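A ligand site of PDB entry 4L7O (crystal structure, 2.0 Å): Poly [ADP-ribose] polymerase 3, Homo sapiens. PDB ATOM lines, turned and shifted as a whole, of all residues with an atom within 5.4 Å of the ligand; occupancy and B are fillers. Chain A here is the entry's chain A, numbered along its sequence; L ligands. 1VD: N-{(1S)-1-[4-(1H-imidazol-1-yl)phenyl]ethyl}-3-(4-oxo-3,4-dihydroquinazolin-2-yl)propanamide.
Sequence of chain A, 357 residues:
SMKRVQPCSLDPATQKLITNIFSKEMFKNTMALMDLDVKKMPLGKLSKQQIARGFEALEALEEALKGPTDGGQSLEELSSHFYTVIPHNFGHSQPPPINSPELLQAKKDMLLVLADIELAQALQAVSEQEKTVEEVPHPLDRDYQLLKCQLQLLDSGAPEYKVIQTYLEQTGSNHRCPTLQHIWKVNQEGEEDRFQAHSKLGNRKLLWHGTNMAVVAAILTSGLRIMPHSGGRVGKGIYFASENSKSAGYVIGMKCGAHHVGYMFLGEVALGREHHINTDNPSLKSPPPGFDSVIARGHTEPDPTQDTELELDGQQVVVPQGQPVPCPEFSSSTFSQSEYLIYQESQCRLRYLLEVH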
ATOM      1  N   ASP A 109      -7.642   2.246  -3.962  1.00  0.00           N
ATOM      2  CA  ASP A 109      -7.350   2.196  -2.519  1.00  0.00           C
ATOM      3  C   ASP A 109      -7.905   0.949  -1.821  1.00  0.00           C
ATOM      4  O   ASP A 109      -7.230   0.363  -1.003  1.00  0.00           O
ATOM      5  CB  ASP A 109      -7.845   3.464  -1.823  1.00  0.00           C
ATOM      6  CG  ASP A 109      -6.997   4.692  -2.147  1.00  0.00           C
ATOM      7  OD1 ASP A 109      -5.918   4.595  -2.821  1.00  0.00           O
ATOM      8  OD2 ASP A 109      -7.398   5.778  -1.679  1.00  0.00           O
ATOM      9  N   LEU A 112      -5.538  -1.878  -2.754  1.00  0.00           N
ATOM     10  CA  LEU A 112      -4.303  -1.675  -1.953  1.00  0.00           C
ATOM     11  C   LEU A 112      -4.458  -2.272  -0.547  1.00  0.00           C
ATOM     12  O   LEU A 112      -3.565  -3.011  -0.067  1.00  0.00           O
ATOM     13  CB  LEU A 112      -3.942  -0.182  -1.910  1.00  0.00           C
ATOM     14  CG  LEU A 112      -3.230   0.381  -3.151  1.00  0.00           C
ATOM     15  CD1 LEU A 112      -3.144   1.945  -3.147  1.00  0.00           C
ATOM     16  CD2 LEU A 112      -1.828  -0.269  -3.322  1.00  0.00           C
ATOM     17  N   VAL A 113      -5.628  -2.036   0.049  1.00  0.00           N
ATOM     18  CA  VAL A 113      -5.953  -2.612   1.361  1.00  0.00           C
ATOM     19  C   VAL A 113      -6.013  -4.149   1.227  1.00  0.00           C
ATOM     20  O   VAL A 113      -5.379  -4.860   1.976  1.00  0.00           O
ATOM     21  CB  VAL A 113      -7.280  -2.032   1.970  1.00  0.00           C
ATOM     22  CG1 VAL A 113      -7.687  -2.830   3.296  1.00  0.00           C
ATOM     23  CG2 VAL A 113      -7.162  -0.501   2.203  1.00  0.00           C
ATOM     24  N   ALA A 115      -4.616  -6.030  -0.993  1.00  0.00           N
ATOM     25  CA  ALA A 115      -3.248  -6.506  -1.212  1.00  0.00           C
ATOM     26  C   ALA A 115      -2.531  -6.751   0.126  1.00  0.00           C
ATOM     27  O   ALA A 115      -1.816  -7.726   0.281  1.00  0.00           O
ATOM     28  CB  ALA A 115      -2.456  -5.473  -2.105  1.00  0.00           C
ATOM     29  N   ASP A 116      -2.752  -5.892   1.106  1.00  0.00           N
ATOM     30  CA  ASP A 116      -2.145  -6.083   2.400  1.00  0.00           C
ATOM     31  C   ASP A 116      -2.837  -7.182   3.233  1.00  0.00           C
ATOM     32  O   ASP A 116      -2.211  -7.823   4.106  1.00  0.00           O
ATOM     33  CB  ASP A 116      -2.055  -4.754   3.158  1.00  0.00           C
ATOM     34  CG  ASP A 116      -0.854  -3.910   2.675  1.00  0.00           C
ATOM     35  OD1 ASP A 116       0.013  -4.475   1.931  1.00  0.00           O
ATOM     36  OD2 ASP A 116      -0.733  -2.726   3.071  1.00  0.00           O
ATOM     37  N   TRP A 208       2.501  11.725  12.060  1.00  0.00           N
ATOM     38  CA  TRP A 208       1.458  10.706  12.182  1.00  0.00           C
ATOM     39  C   TRP A 208       1.169  10.052  10.872  1.00  0.00           C
ATOM     40  O   TRP A 208       1.140  10.711   9.829  1.00  0.00           O
ATOM     41  CB  TRP A 208       0.157  11.321  12.680  1.00  0.00           C
ATOM     42  CG  TRP A 208       0.271  11.946  14.034  1.00  0.00           C
ATOM     43  CD1 TRP A 208       0.415  13.268  14.320  1.00  0.00           C
ATOM     44  CD2 TRP A 208       0.252  11.266  15.301  1.00  0.00           C
ATOM     45  NE1 TRP A 208       0.459  13.455  15.711  1.00  0.00           N
ATOM     46  CE2 TRP A 208       0.402  12.242  16.319  1.00  0.00           C
ATOM     47  CE3 TRP A 208       0.142   9.924  15.670  1.00  0.00           C
ATOM     48  CZ2 TRP A 208       0.451  11.901  17.676  1.00  0.00           C
ATOM     49  CZ3 TRP A 208       0.180   9.598  16.988  1.00  0.00           C
ATOM     50  CH2 TRP A 208       0.362  10.567  17.988  1.00  0.00           C
ATOM     51  N   HIS A 209       0.940   8.739  10.917  1.00  0.00           N
ATOM     52  CA  HIS A 209       0.345   8.030   9.802  1.00  0.00           C
ATOM     53  C   HIS A 209      -0.730   7.107  10.392  1.00  0.00           C
ATOM     54  O   HIS A 209      -0.411   6.111  11.085  1.00  0.00           O
ATOM     55  CB  HIS A 209       1.400   7.259   8.990  1.00  0.00           C
ATOM     56  CG  HIS A 209       0.836   6.529   7.819  1.00  0.00           C
ATOM     57  ND1 HIS A 209       0.769   7.083   6.550  1.00  0.00           N
ATOM     58  CD2 HIS A 209       0.296   5.287   7.718  1.00  0.00           C
ATOM     59  CE1 HIS A 209       0.217   6.211   5.727  1.00  0.00           C
ATOM     60  NE2 HIS A 209      -0.083   5.114   6.407  1.00  0.00           N
ATOM     61  N   GLY A 210      -1.998   7.470  10.204  1.00  0.00           N
ATOM     62  CA  GLY A 210      -3.108   6.619  10.636  1.00  0.00           C
ATOM     63  C   GLY A 210      -3.492   5.616   9.553  1.00  0.00           C
ATOM     64  O   GLY A 210      -3.530   5.962   8.367  1.00  0.00           O
ATOM     65  N   THR A 211      -3.811   4.375   9.893  1.00  0.00           N
ATOM     66  CA  THR A 211      -4.357   3.414   8.901  1.00  0.00           C
ATOM     67  C   THR A 211      -5.470   2.489   9.438  1.00  0.00           C
ATOM     68  O   THR A 211      -5.735   2.534  10.552  1.00  0.00           O
ATOM     69  CB  THR A 211      -3.328   2.421   8.276  1.00  0.00           C
ATOM     70  OG1 THR A 211      -2.760   1.658   9.273  1.00  0.00           O
ATOM     71  CG2 THR A 211      -2.263   3.087   7.369  1.00  0.00           C
ATOM     72  N   ASN A 212      -6.054   1.706   8.526  1.00  0.00           N
ATOM     73  CA  ASN A 212      -6.857   0.526   8.755  1.00  0.00           C
ATOM     74  C   ASN A 212      -6.103  -0.489   9.627  1.00  0.00           C
ATOM     75  O   ASN A 212      -4.984  -0.775   9.385  1.00  0.00           O
ATOM     76  CB  ASN A 212      -7.102  -0.256   7.453  1.00  0.00           C
ATOM     77  CG  ASN A 212      -8.234   0.254   6.613  1.00  0.00           C
ATOM     78  OD1 ASN A 212      -9.323  -0.296   6.632  1.00  0.00           O
ATOM     79  ND2 ASN A 212      -7.958   1.210   5.806  1.00  0.00           N
ATOM     80  N   VAL A 215      -4.169  -3.273   7.599  1.00  0.00           N
ATOM     81  CA  VAL A 215      -2.859  -3.103   6.935  1.00  0.00           C
ATOM     82  C   VAL A 215      -1.692  -2.995   7.936  1.00  0.00           C
ATOM     83  O   VAL A 215      -0.532  -2.774   7.543  1.00  0.00           O
ATOM     84  CB  VAL A 215      -2.823  -1.926   5.943  1.00  0.00           C
ATOM     85  CG1 VAL A 215      -4.029  -1.995   4.991  1.00  0.00           C
ATOM     86  CG2 VAL A 215      -2.693  -0.586   6.631  1.00  0.00           C
ATOM     87  N   ARG A 225       4.850   2.072   2.247  1.00  0.00           N
ATOM     88  CA  ARG A 225       5.217   1.780   0.876  1.00  0.00           C
ATOM     89  C   ARG A 225       4.443   2.646  -0.119  1.00  0.00           C
ATOM     90  O   ARG A 225       3.361   3.135   0.192  1.00  0.00           O
ATOM     91  CB  ARG A 225       4.846   0.310   0.586  1.00  0.00           C
ATOM     92  CG  ARG A 225       5.809  -0.708   1.189  1.00  0.00           C
ATOM     93  CD  ARG A 225       5.102  -2.057   1.616  1.00  0.00           C
ATOM     94  NE  ARG A 225       4.097  -1.756   2.639  1.00  0.00           N
ATOM     95  CZ  ARG A 225       2.887  -2.329   2.721  1.00  0.00           C
ATOM     96  NH1 ARG A 225       2.508  -3.301   1.907  1.00  0.00           N
ATOM     97  NH2 ARG A 225       2.016  -1.880   3.609  1.00  0.00           N
ATOM     98  N   ILE A 226       4.980   2.794  -1.334  1.00  0.00           N
ATOM     99  CA  ILE A 226       4.327   3.487  -2.421  1.00  0.00           C
ATOM    100  C   ILE A 226       4.140   2.439  -3.497  1.00  0.00           C
ATOM    101  O   ILE A 226       5.067   1.712  -3.820  1.00  0.00           O
ATOM    102  CB  ILE A 226       5.238   4.608  -3.015  1.00  0.00           C
ATOM    103  CG1 ILE A 226       5.619   5.619  -1.936  1.00  0.00           C
ATOM    104  CG2 ILE A 226       4.559   5.293  -4.154  1.00  0.00           C
ATOM    105  CD1 ILE A 226       6.706   6.611  -2.338  1.00  0.00           C
ATOM    106  N   MET A 227       2.915   2.347  -4.030  1.00  0.00           N
ATOM    107  CA  MET A 227       2.620   1.426  -5.113  1.00  0.00           C
ATOM    108  C   MET A 227       2.248   2.159  -6.379  1.00  0.00           C
ATOM    109  O   MET A 227       1.936   3.357  -6.377  1.00  0.00           O
ATOM    110  CB  MET A 227       1.515   0.477  -4.729  1.00  0.00           C
ATOM    111  CG  MET A 227       1.934  -0.434  -3.639  1.00  0.00           C
ATOM    112  SD  MET A 227       3.094  -1.690  -4.191  1.00  0.00           S
ATOM    113  CE  MET A 227       1.960  -2.755  -5.150  1.00  0.00           C
ATOM    114  N   SER A 230      -0.890   4.045  -5.939  1.00  0.00           N
ATOM    115  CA  SER A 230      -1.002   4.965  -4.800  1.00  0.00           C
ATOM    116  C   SER A 230      -1.414   6.341  -5.312  1.00  0.00           C
ATOM    117  O   SER A 230      -0.936   6.772  -6.338  1.00  0.00           O
ATOM    118  CB  SER A 230       0.332   5.110  -4.041  1.00  0.00           C
ATOM    119  OG  SER A 230       0.731   3.911  -3.418  1.00  0.00           O
ATOM    120  N   TYR A 239       1.835   9.566   2.742  1.00  0.00           N
ATOM    121  CA  TYR A 239       1.193  10.661   3.412  1.00  0.00           C
ATOM    122  C   TYR A 239       1.322  10.577   4.901  1.00  0.00           C
ATOM    123  O   TYR A 239       1.147   9.509   5.473  1.00  0.00           O
ATOM    124  CB  TYR A 239      -0.310  10.656   3.082  1.00  0.00           C
ATOM    125  CG  TYR A 239      -0.624  11.012   1.623  1.00  0.00           C
ATOM    126  CD1 TYR A 239      -1.122  12.283   1.304  1.00  0.00           C
ATOM    127  CD2 TYR A 239      -0.444  10.093   0.591  1.00  0.00           C
ATOM    128  CE1 TYR A 239      -1.442  12.622  -0.018  1.00  0.00           C
ATOM    129  CE2 TYR A 239      -0.710  10.427  -0.740  1.00  0.00           C
ATOM    130  CZ  TYR A 239      -1.227  11.699  -1.037  1.00  0.00           C
ATOM    131  OH  TYR A 239      -1.495  12.078  -2.343  1.00  0.00           O
ATOM    132  N   PHE A 240       1.585  11.738   5.499  1.00  0.00           N
ATOM    133  CA  PHE A 240       1.654  11.970   6.948  1.00  0.00           C
ATOM    134  C   PHE A 240       0.955  13.268   7.320  1.00  0.00           C
ATOM    135  O   PHE A 240       0.693  14.137   6.485  1.00  0.00           O
ATOM    136  CB  PHE A 240       3.101  12.057   7.450  1.00  0.00           C
ATOM    137  CG  PHE A 240       3.974  10.888   7.112  1.00  0.00           C
ATOM    138  CD1 PHE A 240       4.212   9.908   8.036  1.00  0.00           C
ATOM    139  CD2 PHE A 240       4.630  10.832   5.871  1.00  0.00           C
ATOM    140  CE1 PHE A 240       5.014   8.802   7.726  1.00  0.00           C
ATOM    141  CE2 PHE A 240       5.421   9.783   5.539  1.00  0.00           C
ATOM    142  CZ  PHE A 240       5.642   8.741   6.499  1.00  0.00           C
ATOM    143  N   ALA A 241       0.695  13.429   8.603  1.00  0.00           N
ATOM    144  CA  ALA A 241       0.136  14.661   9.131  1.00  0.00           C
ATOM    145  C   ALA A 241       0.851  15.026  10.417  1.00  0.00           C
ATOM    146  O   ALA A 241       1.236  14.151  11.201  1.00  0.00           O
ATOM    147  CB  ALA A 241      -1.389  14.477   9.434  1.00  0.00           C
ATOM    148  N   LYS A 246      -6.008  14.972  11.840  1.00  0.00           N
ATOM    149  CA  LYS A 246      -6.008  14.667  10.400  1.00  0.00           C
ATOM    150  C   LYS A 246      -5.799  13.161  10.134  1.00  0.00           C
ATOM    151  O   LYS A 246      -6.605  12.499   9.454  1.00  0.00           O
ATOM    152  CB  LYS A 246      -4.924  15.519   9.709  1.00  0.00           C
ATOM    153  CG  LYS A 246      -4.707  15.247   8.223  1.00  0.00           C
ATOM    154  CD  LYS A 246      -5.845  15.844   7.401  1.00  0.00           C
ATOM    155  CE  LYS A 246      -5.855  15.351   5.961  1.00  0.00           C
ATOM    156  NZ  LYS A 246      -5.953  16.499   5.002  1.00  0.00           N
ATOM    157  N   SER A 247      -4.725  12.578  10.681  1.00  0.00           N
ATOM    158  CA  SER A 247      -4.481  11.153  10.554  1.00  0.00           C
ATOM    159  C   SER A 247      -5.533  10.220  11.127  1.00  0.00           C
ATOM    160  O   SER A 247      -5.756   9.130  10.607  1.00  0.00           O
ATOM    161  CB  SER A 247      -3.126  10.842  11.185  1.00  0.00           C
ATOM    162  OG  SER A 247      -2.123  11.342  10.356  1.00  0.00           O
ATOM    163  N   TYR A 250      -8.323   8.787   9.089  1.00  0.00           N
ATOM    164  CA  TYR A 250      -8.052   7.586   8.322  1.00  0.00           C
ATOM    165  C   TYR A 250      -8.107   6.276   9.088  1.00  0.00           C
ATOM    166  O   TYR A 250      -7.985   5.232   8.485  1.00  0.00           O
ATOM    167  CB  TYR A 250      -6.710   7.706   7.614  1.00  0.00           C
ATOM    168  CG  TYR A 250      -6.757   8.817   6.626  1.00  0.00           C
ATOM    169  CD1 TYR A 250      -7.184   8.575   5.334  1.00  0.00           C
ATOM    170  CD2 TYR A 250      -6.453  10.103   6.980  1.00  0.00           C
ATOM    171  CE1 TYR A 250      -7.284   9.587   4.408  1.00  0.00           C
ATOM    172  CE2 TYR A 250      -6.528  11.140   6.066  1.00  0.00           C
ATOM    173  CZ  TYR A 250      -6.954  10.861   4.766  1.00  0.00           C
ATOM    174  OH  TYR A 250      -7.035  11.839   3.822  1.00  0.00           O
ATOM    175  N   SER A 338      -2.307  20.294   7.185  1.00  0.00           N
ATOM    176  CA  SER A 338      -1.169  19.923   6.341  1.00  0.00           C
ATOM    177  C   SER A 338      -1.065  18.433   6.047  1.00  0.00           C
ATOM    178  O   SER A 338      -1.321  17.574   6.933  1.00  0.00           O
ATOM    179  CB  SER A 338       0.141  20.369   7.043  1.00  0.00           C
ATOM    180  OG  SER A 338       0.204  21.784   7.129  1.00  0.00           O
ATOM    181  N   GLU A 339      -0.664  18.124   4.801  1.00  0.00           N
ATOM    182  CA  GLU A 339      -0.302  16.772   4.398  1.00  0.00           C
ATOM    183  C   GLU A 339       1.146  16.839   4.023  1.00  0.00           C
ATOM    184  O   GLU A 339       1.511  17.681   3.187  1.00  0.00           O
ATOM    185  CB  GLU A 339      -1.164  16.294   3.233  1.00  0.00           C
ATOM    186  CG  GLU A 339      -2.679  16.336   3.628  1.00  0.00           C
ATOM    187  CD  GLU A 339      -3.601  15.708   2.665  1.00  0.00           C
ATOM    188  OE1 GLU A 339      -3.105  14.971   1.743  1.00  0.00           O
ATOM    189  OE2 GLU A 339      -4.839  15.940   2.832  1.00  0.00           O
HETATM  190  CAM 1VD L   1       1.205  -0.226  -0.012  1.00  0.00           C
HETATM  191  CAF 1VD L   1       1.765  -1.307  -0.623  1.00  0.00           C
HETATM  192  NAQ 1VD L   1       0.796  -2.237  -0.753  1.00  0.00           N
HETATM  193  CAN 1VD L   1      -0.338  -1.741  -0.261  1.00  0.00           C
HETATM  194  NBC 1VD L   1      -0.094  -0.508   0.222  1.00  0.00           N
HETATM  195  CAW 1VD L   1      -1.076   0.238   0.731  1.00  0.00           C
HETATM  196  CAJ 1VD L   1      -1.170   1.595   0.313  1.00  0.00           C
HETATM  197  CAH 1VD L   1      -2.238   2.364   0.792  1.00  0.00           C
HETATM  198  CAI 1VD L   1      -2.040  -0.300   1.597  1.00  0.00           C
HETATM  199  CAG 1VD L   1      -3.062   0.484   2.069  1.00  0.00           C
HETATM  200  CAV 1VD L   1      -3.183   1.810   1.685  1.00  0.00           C
HETATM  201  CBB 1VD L   1      -4.290   2.598   2.167  1.00  0.00           C
HETATM  202  CAA 1VD L   1      -5.311   2.719   1.019  1.00  0.00           C
HETATM  203  NAS 1VD L   1      -3.942   3.995   2.497  1.00  0.00           N
HETATM  204  CAU 1VD L   1      -3.732   4.422   3.748  1.00  0.00           C
HETATM  205  OAB 1VD L   1      -3.759   3.680   4.727  1.00  0.00           O
HETATM  206  CAO 1VD L   1      -3.464   5.959   3.850  1.00  0.00           C
HETATM  207  CAP 1VD L   1      -3.723   6.398   5.280  1.00  0.00           C
HETATM  208  CAX 1VD L   1      -3.455   7.767   5.503  1.00  0.00           C
HETATM  209  NAR 1VD L   1      -3.636   8.752   4.621  1.00  0.00           N
HETATM  210  CAZ 1VD L   1      -3.323  10.055   4.925  1.00  0.00           C
HETATM  211  CAK 1VD L   1      -3.559  11.056   3.992  1.00  0.00           C
HETATM  212  CAD 1VD L   1      -3.289  12.396   4.314  1.00  0.00           C
HETATM  213  CAE 1VD L   1      -2.814  12.730   5.559  1.00  0.00           C
HETATM  214  CAL 1VD L   1      -2.606  11.727   6.513  1.00  0.00           C
HETATM  215  CBA 1VD L   1      -2.887  10.417   6.191  1.00  0.00           C
HETATM  216  CAY 1VD L   1      -2.691   9.375   7.118  1.00  0.00           C
HETATM  217  OAC 1VD L   1      -2.292   9.551   8.275  1.00  0.00           O
HETATM  218  NAT 1VD L   1      -2.990   8.094   6.740  1.00  0.00           N
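An oxygen (OAC) of the ligand is in hydrogen-bond range of the backbone NH of Gly 210 (2.9 Å).
NAQ of the ligand lies close to NH1 of Arg 225 (3.3 Å).
The backbone carbonyl oxygen (O) of Gly 210 lies within hydrogen-bond range of a nitrogen (NAT) of the ligand, 2.7 Å away.
The side-chain hydroxyl (OG) of Ser 247 lies within hydrogen-bond range of an oxygen (OAC) of the ligand (2.8 Å).
A ring nitrogen (ND1) of His 209 sits at hydrogen-bond distance from the backbone carbonyl oxygen (O) of Tyr 239 (2.7 Å).
OE2 of Glu 339 is in salt-bridge range of NZ of Lys 246 (2.5 Å).
The backbone NH of Trp 208 sits at hydrogen-bond distance from the backbone carbonyl oxygen of Ala 241 (2.9 Å).
The side-chain hydroxyl (OG) of Ser 230 lies within hydrogen-bond range of the backbone NH (N) of Met 227 (2.8 Å).
OG of Ser 247 lies close to O of Trp 208 (3.4 Å).
The side-chain carboxylate (OD1) of Asp 116 lies within salt-bridge range of the guanidinium group (NH1) of Arg 225 (2.8 Å).
Residues that only touch the ligand: Asp 109, Leu 112, Val 113, Asp 116, Trp 208, His 209, Thr 211, Val 215, Met 227, Tyr 239, Phe 240, Tyr 250 and Glu 339.
Hydrophobic or aromatic side chains within 4 Å of the ligand: Leu 112, Val 113, His 209, Val 215, Met 227, Tyr 239 and Tyr 250.
Within 4 Å of the ligand: Asp 109, Leu 112, Val 113, Asp 116, Trp 208, His 209, Gly 210, Thr 211, Val 215, Arg 225, Met 227, Tyr 239, Phe 240, Ser 247, Tyr 250 and Glu 339.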
